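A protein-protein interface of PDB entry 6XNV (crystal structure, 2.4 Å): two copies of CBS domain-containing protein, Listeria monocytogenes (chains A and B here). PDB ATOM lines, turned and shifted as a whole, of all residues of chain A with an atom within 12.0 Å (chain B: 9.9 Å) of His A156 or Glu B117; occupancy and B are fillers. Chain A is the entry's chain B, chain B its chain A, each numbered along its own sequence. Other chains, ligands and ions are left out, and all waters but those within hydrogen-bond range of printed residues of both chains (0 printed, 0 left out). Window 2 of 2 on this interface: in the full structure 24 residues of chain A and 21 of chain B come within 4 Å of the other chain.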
ATOM      1  N   VAL A 147      28.153 -29.750  -4.900  1.00  0.00           N
ATOM      2  CA  VAL A 147      28.271 -28.446  -5.544  1.00  0.00           C
ATOM      3  C   VAL A 147      27.193 -28.266  -6.601  1.00  0.00           C
ATOM      4  O   VAL A 147      26.551 -27.212  -6.677  1.00  0.00           O
ATOM      5  CB  VAL A 147      29.683 -28.271  -6.131  1.00  0.00           C
ATOM      6  CG1 VAL A 147      29.707 -27.102  -7.091  1.00  0.00           C
ATOM      7  CG2 VAL A 147      30.708 -28.070  -5.023  1.00  0.00           C
ATOM      8  N   LEU A 148      26.971 -29.288  -7.429  1.00  0.00           N
ATOM      9  CA  LEU A 148      26.003 -29.158  -8.509  1.00  0.00           C
ATOM     10  C   LEU A 148      24.583 -28.988  -7.987  1.00  0.00           C
ATOM     11  O   LEU A 148      23.758 -28.320  -8.624  1.00  0.00           O
ATOM     12  CB  LEU A 148      26.057 -30.381  -9.404  1.00  0.00           C
ATOM     13  CG  LEU A 148      27.455 -30.484 -10.018  1.00  0.00           C
ATOM     14  CD1 LEU A 148      27.691 -31.891 -10.519  1.00  0.00           C
ATOM     15  CD2 LEU A 148      27.632 -29.446 -11.099  1.00  0.00           C
ATOM     16  N   LYS A 149      24.271 -29.590  -6.839  1.00  0.00           N
ATOM     17  CA  LYS A 149      22.983 -29.326  -6.207  1.00  0.00           C
ATOM     18  C   LYS A 149      22.813 -27.843  -5.918  1.00  0.00           C
ATOM     19  O   LYS A 149      21.753 -27.278  -6.182  1.00  0.00           O
ATOM     20  CB  LYS A 149      22.843 -30.169  -4.938  1.00  0.00           C
ATOM     21  CG  LYS A 149      21.388 -30.364  -4.483  1.00  0.00           C
ATOM     22  CD  LYS A 149      20.445 -30.336  -5.673  1.00  0.00           C
ATOM     23  CE  LYS A 149      19.066 -30.910  -5.358  1.00  0.00           C
ATOM     24  NZ  LYS A 149      18.432 -31.583  -6.561  1.00  0.00           N
ATOM     25  N   GLN A 150      23.853 -27.188  -5.415  1.00  0.00           N
ATOM     26  CA  GLN A 150      23.739 -25.759  -5.145  1.00  0.00           C
ATOM     27  C   GLN A 150      23.658 -24.929  -6.429  1.00  0.00           C
ATOM     28  O   GLN A 150      22.959 -23.911  -6.477  1.00  0.00           O
ATOM     29  CB  GLN A 150      24.912 -25.324  -4.278  1.00  0.00           C
ATOM     30  CG  GLN A 150      24.718 -25.674  -2.809  1.00  0.00           C
ATOM     31  CD  GLN A 150      23.928 -24.595  -2.072  1.00  0.00           C
ATOM     32  OE1 GLN A 150      22.732 -24.405  -2.312  1.00  0.00           O
ATOM     33  NE2 GLN A 150      24.610 -23.858  -1.195  1.00  0.00           N
ATOM     34  N   VAL A 151      24.352 -25.346  -7.484  1.00  0.00           N
ATOM     35  CA  VAL A 151      24.293 -24.612  -8.751  1.00  0.00           C
ATOM     36  C   VAL A 151      22.888 -24.678  -9.340  1.00  0.00           C
ATOM     37  O   VAL A 151      22.330 -23.662  -9.772  1.00  0.00           O
ATOM     38  CB  VAL A 151      25.345 -25.153  -9.747  1.00  0.00           C
ATOM     39  CG1 VAL A 151      24.995 -24.756 -11.174  1.00  0.00           C
ATOM     40  CG2 VAL A 151      26.740 -24.666  -9.405  1.00  0.00           C
ATOM     41  N   ASN A 152      22.302 -25.878  -9.382  1.00  0.00           N
ATOM     42  CA  ASN A 152      20.936 -26.022  -9.882  1.00  0.00           C
ATOM     43  C   ASN A 152      19.942 -25.263  -9.010  1.00  0.00           C
ATOM     44  O   ASN A 152      18.904 -24.795  -9.500  1.00  0.00           O
ATOM     45  CB  ASN A 152      20.567 -27.507  -9.949  1.00  0.00           C
ATOM     46  CG  ASN A 152      19.310 -27.773 -10.756  1.00  0.00           C
ATOM     47  OD1 ASN A 152      19.164 -27.304 -11.888  1.00  0.00           O
ATOM     48  ND2 ASN A 152      18.391 -28.542 -10.173  1.00  0.00           N
ATOM     49  N   ARG A 153      20.250 -25.122  -7.721  1.00  0.00           N
ATOM     50  CA  ARG A 153      19.353 -24.422  -6.808  1.00  0.00           C
ATOM     51  C   ARG A 153      19.285 -22.932  -7.125  1.00  0.00           C
ATOM     52  O   ARG A 153      18.206 -22.333  -7.076  1.00  0.00           O
ATOM     53  CB  ARG A 153      19.812 -24.663  -5.367  1.00  0.00           C
ATOM     54  CG  ARG A 153      18.863 -24.189  -4.304  1.00  0.00           C
ATOM     55  CD  ARG A 153      19.444 -24.426  -2.917  1.00  0.00           C
ATOM     56  NE  ARG A 153      19.865 -25.813  -2.713  1.00  0.00           N
ATOM     57  CZ  ARG A 153      19.036 -26.854  -2.617  1.00  0.00           C
ATOM     58  NH1 ARG A 153      17.726 -26.683  -2.722  1.00  0.00           N
ATOM     59  NH2 ARG A 153      19.515 -28.074  -2.419  1.00  0.00           N
ATOM     60  N   TYR A 154      20.415 -22.316  -7.470  1.00  0.00           N
ATOM     61  CA  TYR A 154      20.422 -20.883  -7.726  1.00  0.00           C
ATOM     62  C   TYR A 154      19.900 -20.514  -9.111  1.00  0.00           C
ATOM     63  O   TYR A 154      19.624 -19.337  -9.352  1.00  0.00           O
ATOM     64  CB  TYR A 154      21.829 -20.310  -7.536  1.00  0.00           C
ATOM     65  CG  TYR A 154      22.353 -20.393  -6.101  1.00  0.00           C
ATOM     66  CD1 TYR A 154      21.487 -20.537  -5.013  1.00  0.00           C
ATOM     67  CD2 TYR A 154      23.724 -20.314  -5.835  1.00  0.00           C
ATOM     68  CE1 TYR A 154      21.983 -20.614  -3.701  1.00  0.00           C
ATOM     69  CE2 TYR A 154      24.224 -20.387  -4.536  1.00  0.00           C
ATOM     70  CZ  TYR A 154      23.360 -20.538  -3.479  1.00  0.00           C
ATOM     71  OH  TYR A 154      23.896 -20.609  -2.211  1.00  0.00           O
ATOM     72  N   ILE A 155      19.736 -21.459 -10.027  1.00  0.00           N
ATOM     73  CA  ILE A 155      19.173 -21.112 -11.332  1.00  0.00           C
ATOM     74  C   ILE A 155      17.651 -21.236 -11.338  1.00  0.00           C
ATOM     75  O   ILE A 155      16.952 -20.309 -11.757  1.00  0.00           O
ATOM     76  CB  ILE A 155      19.830 -21.951 -12.452  1.00  0.00           C
ATOM     77  CG1 ILE A 155      19.320 -23.395 -12.461  1.00  0.00           C
ATOM     78  CG2 ILE A 155      21.346 -21.927 -12.306  1.00  0.00           C
ATOM     79  CD1 ILE A 155      19.153 -23.964 -13.821  1.00  0.00           C
ATOM     80  N   HIS A 156      17.107 -22.350 -10.838  1.00  0.00           N
ATOM     81  CA  HIS A 156      15.663 -22.570 -10.804  1.00  0.00           C
ATOM     82  C   HIS A 156      15.030 -21.729  -9.695  1.00  0.00           C
ATOM     83  O   HIS A 156      15.507 -20.638  -9.364  1.00  0.00           O
ATOM     84  CB  HIS A 156      15.342 -24.064 -10.598  1.00  0.00           C
ATOM     85  CG  HIS A 156      15.410 -24.890 -11.850  1.00  0.00           C
ATOM     86  ND1 HIS A 156      16.121 -26.072 -11.928  1.00  0.00           N
ATOM     87  CD2 HIS A 156      14.837 -24.717 -13.065  1.00  0.00           C
ATOM     88  CE1 HIS A 156      15.990 -26.586 -13.139  1.00  0.00           C
ATOM     89  NE2 HIS A 156      15.217 -25.783 -13.849  1.00  0.00           N
ATOM     90  N   ASN B  25      23.414 -19.251 -22.059  1.00  0.00           N
ATOM     91  CA  ASN B  25      24.570 -20.105 -21.820  1.00  0.00           C
ATOM     92  C   ASN B  25      25.272 -20.551 -23.109  1.00  0.00           C
ATOM     93  O   ASN B  25      24.857 -20.231 -24.229  1.00  0.00           O
ATOM     94  CB  ASN B  25      24.159 -21.341 -21.013  1.00  0.00           C
ATOM     95  CG  ASN B  25      24.533 -21.233 -19.546  1.00  0.00           C
ATOM     96  OD1 ASN B  25      25.644 -20.821 -19.198  1.00  0.00           O
ATOM     97  ND2 ASN B  25      23.603 -21.613 -18.674  1.00  0.00           N
ATOM     98  N   GLU B  26      26.349 -21.307 -22.913  1.00  0.00           N
ATOM     99  CA  GLU B  26      27.234 -21.773 -23.973  1.00  0.00           C
ATOM    100  C   GLU B  26      27.372 -23.292 -23.946  1.00  0.00           C
ATOM    101  O   GLU B  26      28.300 -23.838 -24.556  1.00  0.00           O
ATOM    102  CB  GLU B  26      28.608 -21.116 -23.833  1.00  0.00           C
ATOM    103  CG  GLU B  26      29.286 -21.370 -22.472  1.00  0.00           C
ATOM    104  CD  GLU B  26      28.629 -20.614 -21.314  1.00  0.00           C
ATOM    105  OE1 GLU B  26      28.827 -21.021 -20.148  1.00  0.00           O
ATOM    106  OE2 GLU B  26      27.896 -19.627 -21.569  1.00  0.00           O
ATOM    107  N   LEU B  27      26.458 -23.970 -23.242  1.00  0.00           N
ATOM    108  CA  LEU B  27      26.559 -25.407 -23.002  1.00  0.00           C
ATOM    109  C   LEU B  27      26.772 -26.191 -24.293  1.00  0.00           C
ATOM    110  O   LEU B  27      27.552 -27.151 -24.322  1.00  0.00           O
ATOM    111  CB  LEU B  27      25.291 -25.879 -22.289  1.00  0.00           C
ATOM    112  CG  LEU B  27      25.375 -26.915 -21.166  1.00  0.00           C
ATOM    113  CD1 LEU B  27      26.639 -26.731 -20.366  1.00  0.00           C
ATOM    114  CD2 LEU B  27      24.153 -26.782 -20.256  1.00  0.00           C
ATOM    115  N   ILE B 110      20.031 -35.772 -24.366  1.00  0.00           N
ATOM    116  CA  ILE B 110      19.811 -34.415 -24.848  1.00  0.00           C
ATOM    117  C   ILE B 110      19.394 -34.491 -26.312  1.00  0.00           C
ATOM    118  O   ILE B 110      20.157 -34.979 -27.157  1.00  0.00           O
ATOM    119  CB  ILE B 110      21.073 -33.546 -24.715  1.00  0.00           C
ATOM    120  CG1 ILE B 110      21.719 -33.673 -23.339  1.00  0.00           C
ATOM    121  CG2 ILE B 110      20.746 -32.085 -25.024  1.00  0.00           C
ATOM    122  CD1 ILE B 110      20.833 -33.219 -22.239  1.00  0.00           C
ATOM    123  N   ASP B 112      18.265 -31.443 -27.763  1.00  0.00           N
ATOM    124  CA  ASP B 112      18.475 -30.085 -28.244  1.00  0.00           C
ATOM    125  C   ASP B 112      19.040 -29.266 -27.097  1.00  0.00           C
ATOM    126  O   ASP B 112      19.052 -29.702 -25.949  1.00  0.00           O
ATOM    127  CB  ASP B 112      17.167 -29.464 -28.748  1.00  0.00           C
ATOM    128  CG  ASP B 112      16.076 -29.481 -27.689  1.00  0.00           C
ATOM    129  OD1 ASP B 112      16.125 -28.639 -26.759  1.00  0.00           O
ATOM    130  OD2 ASP B 112      15.182 -30.357 -27.777  1.00  0.00           O
ATOM    131  N   PHE B 113      19.451 -28.044 -27.407  1.00  0.00           N
ATOM    132  CA  PHE B 113      19.962 -27.147 -26.382  1.00  0.00           C
ATOM    133  C   PHE B 113      19.023 -25.969 -26.133  1.00  0.00           C
ATOM    134  O   PHE B 113      19.470 -24.851 -25.856  1.00  0.00           O
ATOM    135  CB  PHE B 113      21.369 -26.690 -26.749  1.00  0.00           C
ATOM    136  CG  PHE B 113      22.376 -27.803 -26.689  1.00  0.00           C
ATOM    137  CD1 PHE B 113      22.411 -28.782 -27.673  1.00  0.00           C
ATOM    138  CD2 PHE B 113      23.255 -27.906 -25.623  1.00  0.00           C
ATOM    139  CE1 PHE B 113      23.326 -29.821 -27.614  1.00  0.00           C
ATOM    140  CE2 PHE B 113      24.176 -28.951 -25.562  1.00  0.00           C
ATOM    141  CZ  PHE B 113      24.206 -29.906 -26.560  1.00  0.00           C
ATOM    142  N   ASN B 114      17.709 -26.221 -26.207  1.00  0.00           N
ATOM    143  CA  ASN B 114      16.713 -25.205 -25.879  1.00  0.00           C
ATOM    144  C   ASN B 114      16.420 -25.141 -24.387  1.00  0.00           C
ATOM    145  O   ASN B 114      16.013 -24.084 -23.890  1.00  0.00           O
ATOM    146  CB  ASN B 114      15.404 -25.471 -26.626  1.00  0.00           C
ATOM    147  CG  ASN B 114      15.603 -25.649 -28.120  1.00  0.00           C
ATOM    148  OD1 ASN B 114      16.536 -25.099 -28.706  1.00  0.00           O
ATOM    149  ND2 ASN B 114      14.711 -26.415 -28.750  1.00  0.00           N
ATOM    150  N   ASN B 115      16.602 -26.251 -23.666  1.00  0.00           N
ATOM    151  CA  ASN B 115      16.264 -26.328 -22.248  1.00  0.00           C
ATOM    152  C   ASN B 115      17.494 -26.672 -21.410  1.00  0.00           C
ATOM    153  O   ASN B 115      17.524 -27.705 -20.728  1.00  0.00           O
ATOM    154  CB  ASN B 115      15.162 -27.376 -22.034  1.00  0.00           C
ATOM    155  CG  ASN B 115      14.549 -27.312 -20.648  1.00  0.00           C
ATOM    156  OD1 ASN B 115      14.867 -26.419 -19.854  1.00  0.00           O
ATOM    157  ND2 ASN B 115      13.667 -28.255 -20.348  1.00  0.00           N
ATOM    158  N   ASN B 116      18.509 -25.807 -21.429  1.00  0.00           N
ATOM    159  CA  ASN B 116      19.779 -26.152 -20.796  1.00  0.00           C
ATOM    160  C   ASN B 116      19.701 -26.172 -19.270  1.00  0.00           C
ATOM    161  O   ASN B 116      20.575 -26.763 -18.617  1.00  0.00           O
ATOM    162  CB  ASN B 116      20.864 -25.196 -21.284  1.00  0.00           C
ATOM    163  CG  ASN B 116      21.256 -25.464 -22.727  1.00  0.00           C
ATOM    164  OD1 ASN B 116      22.087 -24.757 -23.307  1.00  0.00           O
ATOM    165  ND2 ASN B 116      20.656 -26.503 -23.314  1.00  0.00           N
ATOM    166  N   GLU B 117      18.673 -25.567 -18.678  1.00  0.00           N
ATOM    167  CA  GLU B 117      18.499 -25.749 -17.244  1.00  0.00           C
ATOM    168  C   GLU B 117      18.049 -27.170 -16.915  1.00  0.00           C
ATOM    169  O   GLU B 117      18.263 -27.638 -15.790  1.00  0.00           O
ATOM    170  CB  GLU B 117      17.534 -24.689 -16.690  1.00  0.00           C
ATOM    171  CG  GLU B 117      16.054 -24.904 -16.951  1.00  0.00           C
ATOM    172  CD  GLU B 117      15.555 -24.175 -18.199  1.00  0.00           C
ATOM    173  OE1 GLU B 117      14.338 -23.891 -18.275  1.00  0.00           O
ATOM    174  OE2 GLU B 117      16.369 -23.909 -19.114  1.00  0.00           O
ATOM    175  N   ARG B 118      17.467 -27.886 -17.880  1.00  0.00           N
ATOM    176  CA  ARG B 118      17.288 -29.320 -17.689  1.00  0.00           C
ATOM    177  C   ARG B 118      18.633 -30.041 -17.669  1.00  0.00           C
ATOM    178  O   ARG B 118      18.811 -31.015 -16.925  1.00  0.00           O
ATOM    179  CB  ARG B 118      16.392 -29.907 -18.779  1.00  0.00           C
ATOM    180  CG  ARG B 118      16.347 -31.439 -18.778  1.00  0.00           C
ATOM    181  CD  ARG B 118      15.377 -31.994 -19.812  1.00  0.00           C
ATOM    182  NE  ARG B 118      15.460 -33.451 -19.850  1.00  0.00           N
ATOM    183  CZ  ARG B 118      16.163 -34.128 -20.752  1.00  0.00           C
ATOM    184  NH1 ARG B 118      16.835 -33.477 -21.696  1.00  0.00           N
ATOM    185  NH2 ARG B 118      16.210 -35.454 -20.709  1.00  0.00           N
ATOM    186  N   ILE B 119      19.590 -29.575 -18.474  1.00  0.00           N
ATOM    187  CA  ILE B 119      20.908 -30.205 -18.494  1.00  0.00           C
ATOM    188  C   ILE B 119      21.627 -29.990 -17.162  1.00  0.00           C
ATOM    189  O   ILE B 119      22.259 -30.912 -16.624  1.00  0.00           O
ATOM    190  CB  ILE B 119      21.729 -29.686 -19.690  1.00  0.00           C
ATOM    191  CG1 ILE B 119      20.980 -29.961 -21.003  1.00  0.00           C
ATOM    192  CG2 ILE B 119      23.091 -30.332 -19.719  1.00  0.00           C
ATOM    193  CD1 ILE B 119      21.681 -29.447 -22.263  1.00  0.00           C
ATOM    194  N   VAL B 120      21.508 -28.796 -16.580  1.00  0.00           N
ATOM    195  CA  VAL B 120      22.090 -28.595 -15.256  1.00  0.00           C
ATOM    196  C   VAL B 120      21.404 -29.486 -14.227  1.00  0.00           C
ATOM    197  O   VAL B 120      22.062 -30.064 -13.349  1.00  0.00           O
ATOM    198  CB  VAL B 120      22.035 -27.110 -14.861  1.00  0.00           C
ATOM    199  CG1 VAL B 120      22.639 -26.915 -13.479  1.00  0.00           C
ATOM    200  CG2 VAL B 120      22.769 -26.282 -15.884  1.00  0.00           C
ATOM    201  N   HIS B 121      20.087 -29.660 -14.346  1.00  0.00           N
ATOM    202  CA  HIS B 121      19.358 -30.495 -13.394  1.00  0.00           C
ATOM    203  C   HIS B 121      19.771 -31.969 -13.485  1.00  0.00           C
ATOM    204  O   HIS B 121      19.820 -32.668 -12.468  1.00  0.00           O
ATOM    205  CB  HIS B 121      17.852 -30.325 -13.617  1.00  0.00           C
ATOM    206  CG  HIS B 121      17.001 -31.143 -12.699  1.00  0.00           C
ATOM    207  ND1 HIS B 121      17.013 -30.982 -11.329  1.00  0.00           N
ATOM    208  CD2 HIS B 121      16.110 -32.131 -12.954  1.00  0.00           C
ATOM    209  CE1 HIS B 121      16.169 -31.838 -10.778  1.00  0.00           C
ATOM    210  NE2 HIS B 121      15.604 -32.545 -11.742  1.00  0.00           N
ATOM    211  N   LEU B 122      20.056 -32.475 -14.686  1.00  0.00           N
ATOM    212  CA  LEU B 122      20.405 -33.893 -14.789  1.00  0.00           C
ATOM    213  C   LEU B 122      21.816 -34.161 -14.269  1.00  0.00           C
ATOM    214  O   LEU B 122      22.075 -35.232 -13.700  1.00  0.00           O
ATOM    215  CB  LEU B 122      20.281 -34.362 -16.237  1.00  0.00           C
ATOM    216  CG  LEU B 122      18.879 -34.471 -16.857  1.00  0.00           C
ATOM    217  CD1 LEU B 122      18.940 -34.301 -18.369  1.00  0.00           C
ATOM    218  CD2 LEU B 122      18.190 -35.794 -16.486  1.00  0.00           C
ATOM    219  N   LEU B 123      22.735 -33.203 -14.462  1.00  0.00           N
ATOM    220  CA  LEU B 123      24.106 -33.358 -14.010  1.00  0.00           C
ATOM    221  C   LEU B 123      24.187 -33.516 -12.504  1.00  0.00           C
ATOM    222  O   LEU B 123      25.184 -34.035 -11.999  1.00  0.00           O
ATOM    223  CB  LEU B 123      24.955 -32.166 -14.470  1.00  0.00           C
ATOM    224  CG  LEU B 123      25.210 -32.218 -15.979  1.00  0.00           C
ATOM    225  CD1 LEU B 123      25.948 -30.997 -16.421  1.00  0.00           C
ATOM    226  CD2 LEU B 123      25.990 -33.473 -16.382  1.00  0.00           C
ATOM    227  N   VAL B 124      23.149 -33.091 -11.786  1.00  0.00           N
ATOM    228  CA  VAL B 124      23.047 -33.386 -10.363  1.00  0.00           C
ATOM    229  C   VAL B 124      23.176 -34.881 -10.128  1.00  0.00           C
ATOM    230  O   VAL B 124      23.897 -35.330  -9.225  1.00  0.00           O
ATOM    231  CB  VAL B 124      21.712 -32.848  -9.811  1.00  0.00           C
ATOM    232  CG1 VAL B 124      21.428 -33.430  -8.426  1.00  0.00           C
ATOM    233  CG2 VAL B 124      21.716 -31.318  -9.787  1.00  0.00           C
ATOM    234  N   VAL B 147      30.359 -27.910 -16.449  1.00  0.00           N
ATOM    235  CA  VAL B 147      29.676 -26.975 -15.557  1.00  0.00           C
ATOM    236  C   VAL B 147      30.613 -26.539 -14.436  1.00  0.00           C
ATOM    237  O   VAL B 147      30.639 -25.370 -14.041  1.00  0.00           O
ATOM    238  CB  VAL B 147      28.375 -27.581 -15.001  1.00  0.00           C
ATOM    239  CG1 VAL B 147      27.835 -26.707 -13.867  1.00  0.00           C
ATOM    240  CG2 VAL B 147      27.343 -27.682 -16.089  1.00  0.00           C
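ND1 of His B121 lies within hydrogen-bond range of ND2 of Asn A152, at 3.0 Å.
Of the 18 printed residues of chain B, 6 touch a printed residue of chain A. Printed residues of chain B that touch a printed residue of chain A: Glu B117, Val B120, His B121, Leu B123, Val B124 and Val B147. Hydrophobic or aromatic side chains of chain B within 4 Å of the printed part of chain A: Val B120, His B121, Val B124 and Val B147. Along chain B the printed residues that touch a printed residue of chain A span positions 117 to 147. Of the 10 printed residues of chain A, 6 touch a printed residue of chain B. Printed residues of chain A that touch a printed residue of chain B: Leu A148, Lys A149, Val A151, Asn A152, Ile A155 and His A156. Among the printed residues, 10 pairs touch across the chains. Among the printed residues, no Asp or Glu carboxylate lies within 4 Å of a Lys or Arg side-chain nitrogen of the other chain.
His A156 touches just one residue of chain B: Glu B117 (3.3 Å). Of the printed residues of chain A, Glu B117 touches Ile A155 (3.4 Å) and His A156 (3.3 Å). Printed residues of chain B within 4 Å of Ile A155: Glu B117. No residue of chain A comes within 4 Å of Asn B115. No residue of chain A comes within 4 Å of Asn B116. Ile B119 touches none of the printed residues of chain A. Val B120 touches just these residues of chain A: Val A151 (3.9 Å) and Asn A152 (3.8 Å). His B121 touches one residue of chain A. Of the printed residues of chain B, Asn A152 touches Val B120, His B121 and Val B124. Of the printed residues of chain A, Val B147 touches Leu A148. Of the printed residues of chain A, Val B124 touches Leu A148 (3.8 Å), Lys A149 (3.98 Å) and Asn A152 (3.98 Å). Asn B114 touches none of the printed residues of chain A. Val A147 touches none of the printed residues of chain B. The nearest residue of chain B that does not touch His A156 is His B121 (4.2 Å). The nearest printed residue of chain A that does not touch Val B124 is Gln A150 (6.4 Å).
The side-chain amide oxygen of Asn A152 sits at hydrogen-bond distance from a ring nitrogen (ND1) of His A156 (3.3 Å). OD1 of Asn B115 lies close to OE2 of Glu B117 (3.0 Å).
Among the printed residues, merely in contact across the chains: Leu A148 with Leu B123, Leu A148 with Val B124, Leu A148 with Val B147, Lys A149 with Val B124, Val A151 with Val B120, Asn A152 with Val B120, Asn A152 with Val B124, Ile A155 with Glu B117 and His A156 with Glu B117.
Position printed for both chains: 147. Of the 10 pairs that touch across the chains among the printed residues, none has its exchanged pair printed and touching as well.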
